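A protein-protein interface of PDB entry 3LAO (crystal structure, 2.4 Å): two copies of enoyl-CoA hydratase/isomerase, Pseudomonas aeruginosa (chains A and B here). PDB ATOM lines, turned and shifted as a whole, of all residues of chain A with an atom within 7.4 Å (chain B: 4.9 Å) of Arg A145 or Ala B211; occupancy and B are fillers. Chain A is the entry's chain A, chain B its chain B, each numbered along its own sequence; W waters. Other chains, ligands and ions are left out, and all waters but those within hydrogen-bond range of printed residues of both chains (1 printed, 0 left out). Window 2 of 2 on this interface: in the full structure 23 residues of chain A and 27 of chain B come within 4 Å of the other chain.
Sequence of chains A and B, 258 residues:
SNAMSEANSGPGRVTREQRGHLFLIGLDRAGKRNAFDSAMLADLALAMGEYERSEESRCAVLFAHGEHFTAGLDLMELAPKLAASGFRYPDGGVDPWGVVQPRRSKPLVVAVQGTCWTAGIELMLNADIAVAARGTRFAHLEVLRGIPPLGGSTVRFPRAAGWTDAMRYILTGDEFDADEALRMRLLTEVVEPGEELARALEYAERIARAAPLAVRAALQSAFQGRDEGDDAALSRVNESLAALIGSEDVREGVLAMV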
ATOM      1  N   LEU A  75       7.244  26.774   6.173  1.00  0.00           N
ATOM      2  CA  LEU A  75       6.437  25.886   5.307  1.00  0.00           C
ATOM      3  C   LEU A  75       5.167  26.519   4.767  1.00  0.00           C
ATOM      4  O   LEU A  75       4.676  26.087   3.738  1.00  0.00           O
ATOM      5  CB  LEU A  75       6.024  24.616   6.058  1.00  0.00           C
ATOM      6  CG  LEU A  75       7.172  23.829   6.669  1.00  0.00           C
ATOM      7  CD1 LEU A  75       6.676  22.877   7.787  1.00  0.00           C
ATOM      8  CD2 LEU A  75       7.902  23.125   5.518  1.00  0.00           C
ATOM      9  N   HIS A 140      15.386  17.552  15.484  1.00  0.00           N
ATOM     10  CA  HIS A 140      14.727  17.146  14.261  1.00  0.00           C
ATOM     11  C   HIS A 140      13.221  16.993  14.467  1.00  0.00           C
ATOM     12  O   HIS A 140      12.662  15.926  14.189  1.00  0.00           O
ATOM     13  CB  HIS A 140      15.305  15.835  13.765  1.00  0.00           C
ATOM     14  CG  HIS A 140      16.586  15.984  12.991  1.00  0.00           C
ATOM     15  ND1 HIS A 140      16.633  16.534  11.725  1.00  0.00           N
ATOM     16  CD2 HIS A 140      17.865  15.639  13.300  1.00  0.00           C
ATOM     17  CE1 HIS A 140      17.882  16.520  11.285  1.00  0.00           C
ATOM     18  NE2 HIS A 140      18.647  15.977  12.220  1.00  0.00           N
ATOM     19  N   LEU A 141      12.565  18.060  14.930  1.00  0.00           N
ATOM     20  CA  LEU A 141      11.113  18.077  15.077  1.00  0.00           C
ATOM     21  C   LEU A 141      10.354  17.552  13.862  1.00  0.00           C
ATOM     22  O   LEU A 141       9.247  17.018  14.021  1.00  0.00           O
ATOM     23  CB  LEU A 141      10.607  19.488  15.360  1.00  0.00           C
ATOM     24  CG  LEU A 141      11.357  20.037  16.540  1.00  0.00           C
ATOM     25  CD1 LEU A 141      10.907  21.445  16.741  1.00  0.00           C
ATOM     26  CD2 LEU A 141      11.145  19.124  17.779  1.00  0.00           C
ATOM     27  N   GLU A 142      10.912  17.710  12.663  1.00  0.00           N
ATOM     28  CA  GLU A 142      10.182  17.267  11.456  1.00  0.00           C
ATOM     29  C   GLU A 142       9.867  15.758  11.394  1.00  0.00           C
ATOM     30  O   GLU A 142       8.871  15.388  10.781  1.00  0.00           O
ATOM     31  CB  GLU A 142      10.832  17.769  10.139  1.00  0.00           C
ATOM     32  CG  GLU A 142      12.110  17.015   9.700  1.00  0.00           C
ATOM     33  CD  GLU A 142      13.349  17.310  10.592  1.00  0.00           C
ATOM     34  OE1 GLU A 142      13.240  18.067  11.591  1.00  0.00           O
ATOM     35  OE2 GLU A 142      14.444  16.797  10.276  1.00  0.00           O
ATOM     36  N   VAL A 143      10.691  14.876  11.983  1.00  0.00           N
ATOM     37  CA  VAL A 143      10.311  13.463  11.943  1.00  0.00           C
ATOM     38  C   VAL A 143       8.967  13.222  12.595  1.00  0.00           C
ATOM     39  O   VAL A 143       8.406  12.124  12.409  1.00  0.00           O
ATOM     40  CB  VAL A 143      11.245  12.438  12.707  1.00  0.00           C
ATOM     41  CG1 VAL A 143      12.446  12.103  11.943  1.00  0.00           C
ATOM     42  CG2 VAL A 143      11.519  12.867  14.136  1.00  0.00           C
ATOM     43  N   LEU A 144       8.506  14.174  13.420  1.00  0.00           N
ATOM     44  CA  LEU A 144       7.169  14.082  14.047  1.00  0.00           C
ATOM     45  C   LEU A 144       6.044  14.439  13.065  1.00  0.00           C
ATOM     46  O   LEU A 144       4.899  14.109  13.286  1.00  0.00           O
ATOM     47  CB  LEU A 144       7.046  14.909  15.355  1.00  0.00           C
ATOM     48  CG  LEU A 144       8.170  14.631  16.406  1.00  0.00           C
ATOM     49  CD1 LEU A 144       8.224  15.639  17.551  1.00  0.00           C
ATOM     50  CD2 LEU A 144       8.172  13.209  16.973  1.00  0.00           C
ATOM     51  N   ARG A 145       6.391  15.062  11.949  1.00  0.00           N
ATOM     52  CA  ARG A 145       5.382  15.642  11.102  1.00  0.00           C
ATOM     53  C   ARG A 145       5.260  14.917   9.786  1.00  0.00           C
ATOM     54  O   ARG A 145       4.181  14.503   9.397  1.00  0.00           O
ATOM     55  CB  ARG A 145       5.677  17.134  10.890  1.00  0.00           C
ATOM     56  CG  ARG A 145       4.698  17.813   9.929  1.00  0.00           C
ATOM     57  CD  ARG A 145       4.607  19.282  10.205  1.00  0.00           C
ATOM     58  NE  ARG A 145       3.975  19.500  11.518  1.00  0.00           N
ATOM     59  CZ  ARG A 145       4.061  20.623  12.246  1.00  0.00           C
ATOM     60  NH1 ARG A 145       4.790  21.665  11.838  1.00  0.00           N
ATOM     61  NH2 ARG A 145       3.435  20.693  13.410  1.00  0.00           N
ATOM     62  N   GLY A 146       6.364  14.778   9.080  1.00  0.00           N
ATOM     63  CA  GLY A 146       6.343  14.207   7.734  1.00  0.00           C
ATOM     64  C   GLY A 146       7.667  14.615   7.102  1.00  0.00           C
ATOM     65  O   GLY A 146       8.429  15.383   7.696  1.00  0.00           O
ATOM     66  N   ILE A 147       7.935  14.100   5.912  1.00  0.00           N
ATOM     67  CA  ILE A 147       9.174  14.350   5.192  1.00  0.00           C
ATOM     68  C   ILE A 147       9.241  15.809   4.756  1.00  0.00           C
ATOM     69  O   ILE A 147       8.307  16.341   4.196  1.00  0.00           O
ATOM     70  CB  ILE A 147       9.273  13.430   3.961  1.00  0.00           C
ATOM     71  CG1 ILE A 147       9.376  11.964   4.391  1.00  0.00           C
ATOM     72  CG2 ILE A 147      10.454  13.778   3.119  1.00  0.00           C
ATOM     73  CD1 ILE A 147       9.117  11.000   3.260  1.00  0.00           C
ATOM     74  N   PRO A 148      10.351  16.467   5.033  1.00  0.00           N
ATOM     75  CA  PRO A 148      10.369  17.880   4.683  1.00  0.00           C
ATOM     76  C   PRO A 148      10.800  18.045   3.244  1.00  0.00           C
ATOM     77  O   PRO A 148      11.427  17.134   2.703  1.00  0.00           O
ATOM     78  CB  PRO A 148      11.450  18.462   5.596  1.00  0.00           C
ATOM     79  CG  PRO A 148      12.186  17.271   6.218  1.00  0.00           C
ATOM     80  CD  PRO A 148      11.614  16.005   5.620  1.00  0.00           C
ATOM     81  N   LEU A 171      15.370   9.727  14.761  1.00  0.00           N
ATOM     82  CA  LEU A 171      14.093   9.011  14.706  1.00  0.00           C
ATOM     83  C   LEU A 171      13.073   9.428  15.778  1.00  0.00           C
ATOM     84  O   LEU A 171      11.940   9.032  15.705  1.00  0.00           O
ATOM     85  CB  LEU A 171      14.312   7.492  14.755  1.00  0.00           C
ATOM     86  CG  LEU A 171      15.398   6.993  13.788  1.00  0.00           C
ATOM     87  CD1 LEU A 171      15.570   5.468  13.886  1.00  0.00           C
ATOM     88  CD2 LEU A 171      15.060   7.392  12.379  1.00  0.00           C
ATOM     89  N   ARG B 209       6.153   7.234  18.093  1.00  0.00           N
ATOM     90  CA  ARG B 209       5.304   8.411  18.042  1.00  0.00           C
ATOM     91  C   ARG B 209       5.672   9.315  16.871  1.00  0.00           C
ATOM     92  O   ARG B 209       4.861  10.143  16.436  1.00  0.00           O
ATOM     93  CB  ARG B 209       5.235   9.164  19.378  1.00  0.00           C
ATOM     94  CG  ARG B 209       4.092   8.639  20.277  1.00  0.00           C
ATOM     95  CD  ARG B 209       3.296   9.769  20.961  1.00  0.00           C
ATOM     96  NE  ARG B 209       2.667  10.675  20.003  1.00  0.00           N
ATOM     97  CZ  ARG B 209       2.946  11.971  19.901  1.00  0.00           C
ATOM     98  NH1 ARG B 209       3.846  12.524  20.704  1.00  0.00           N
ATOM     99  NH2 ARG B 209       2.321  12.719  19.000  1.00  0.00           N
ATOM    100  N   ALA B 210       6.874   9.121  16.337  1.00  0.00           N
ATOM    101  CA  ALA B 210       7.280   9.853  15.140  1.00  0.00           C
ATOM    102  C   ALA B 210       6.379   9.492  13.930  1.00  0.00           C
ATOM    103  O   ALA B 210       5.717   8.469  13.917  1.00  0.00           O
ATOM    104  CB  ALA B 210       8.747   9.570  14.835  1.00  0.00           C
ATOM    105  N   ALA B 211       6.351  10.343  12.918  1.00  0.00           N
ATOM    106  CA  ALA B 211       5.671  10.006  11.675  1.00  0.00           C
ATOM    107  C   ALA B 211       6.391   8.894  10.900  1.00  0.00           C
ATOM    108  O   ALA B 211       7.586   9.029  10.547  1.00  0.00           O
ATOM    109  CB  ALA B 211       5.532  11.282  10.785  1.00  0.00           C
ATOM    110  N   PRO B 212       5.668   7.803  10.598  1.00  0.00           N
ATOM    111  CA  PRO B 212       6.305   6.603  10.011  1.00  0.00           C
ATOM    112  C   PRO B 212       6.954   6.875   8.662  1.00  0.00           C
ATOM    113  O   PRO B 212       8.072   6.426   8.430  1.00  0.00           O
ATOM    114  CB  PRO B 212       5.145   5.590   9.891  1.00  0.00           C
ATOM    115  CG  PRO B 212       4.107   6.095  10.882  1.00  0.00           C
ATOM    116  CD  PRO B 212       4.237   7.604  10.880  1.00  0.00           C
ATOM    117  N   LEU B 213       6.291   7.609   7.782  1.00  0.00           N
ATOM    118  CA  LEU B 213       6.930   7.963   6.522  1.00  0.00           C
ATOM    119  C   LEU B 213       8.229   8.765   6.725  1.00  0.00           C
ATOM    120  O   LEU B 213       9.240   8.603   6.004  1.00  0.00           O
ATOM    121  CB  LEU B 213       5.983   8.762   5.653  1.00  0.00           C
ATOM    122  CG  LEU B 213       4.889   7.968   4.958  1.00  0.00           C
ATOM    123  CD1 LEU B 213       4.203   8.933   4.039  1.00  0.00           C
ATOM    124  CD2 LEU B 213       5.489   6.824   4.176  1.00  0.00           C
ATOM    125  N   ALA B 214       8.207   9.648   7.701  1.00  0.00           N
ATOM    126  CA  ALA B 214       9.381  10.474   7.911  1.00  0.00           C
ATOM    127  C   ALA B 214      10.503   9.607   8.529  1.00  0.00           C
ATOM    128  O   ALA B 214      11.651   9.734   8.130  1.00  0.00           O
ATOM    129  CB  ALA B 214       9.037  11.713   8.771  1.00  0.00           C
ATOM    130  N   VAL B 215      10.148   8.701   9.452  1.00  0.00           N
ATOM    131  CA  VAL B 215      11.102   7.788  10.063  1.00  0.00           C
ATOM    132  C   VAL B 215      11.758   6.920   8.960  1.00  0.00           C
ATOM    133  O   VAL B 215      12.998   6.863   8.821  1.00  0.00           O
ATOM    134  CB  VAL B 215      10.468   6.910  11.185  1.00  0.00           C
ATOM    135  CG1 VAL B 215      11.323   5.652  11.455  1.00  0.00           C
ATOM    136  CG2 VAL B 215      10.262   7.698  12.458  1.00  0.00           C
HETATM  137  O   HOH W   1       3.842  12.450  15.358  1.00  0.00           O
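No position is printed for both chains.
Among the printed residues, pairs that only touch across the chains: Val A143 with Ala B210 (3.5 Å), Val A143 with Ala B214 (3.7 Å), Leu A144 with Ala B210 (3.9 Å), Leu A144 with Ala B211 (3.8 Å), Arg A145 with Ala B211 (3.8 Å), Gly A146 with Ala B211 (3.98 Å), Gly A146 with Ala B214 (3.6 Å), Ile A147 with Leu B213 (3.6 Å), Ile A147 with Ala B214 (3.8 Å), Leu A171 with Ala B210 (3.4 Å) and Leu A171 with Val B215 (3.9 Å).
The backbone carbonyl oxygen of Val A143 is in hydrogen-bond range of the backbone NH of Ala B211 (2.8 Å).
Printed residues of chain B that touch a printed residue of chain A: Ala B210, Ala B211, Leu B213, Ala B214 and Val B215.
Hydrophobic or aromatic side chains of chain A that line the printed part of chain B: Leu A144 and Ile A147.
Along chain A the printed residues that touch a printed residue of chain B span positions 143 to 171.
Among the printed residues, no Asp or Glu carboxylate lies within 4 Å of a Lys or Arg side-chain nitrogen of the other chain.
Arg A145 touches just one residue of chain B: Ala B211 (3.8 Å).
Of chain A, only Val A143, Leu A144, Arg A145 and Gly A146 come within 4 Å of Ala B211.
Of the printed residues of chain A, Leu B213 touches Ile A147.
Printed residues of chain A within 4 Å of Ala B214: Val A143, Gly A146 and Ile A147.
Of the printed residues of chain B, Val A143 touches Ala B210, Ala B211 and Ala B214.
Of the printed residues of chain B, Leu A144 touches Ala B210 (3.9 Å) and Ala B211 (3.8 Å).
Arg B209 touches none of the printed residues of chain A.
The nearest printed residue of chain B that does not touch Arg A145 is Ala B214 (5.1 Å).
Water W1 lies within hydrogen-bond range of O of Arg B209 and O of Leu A144.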
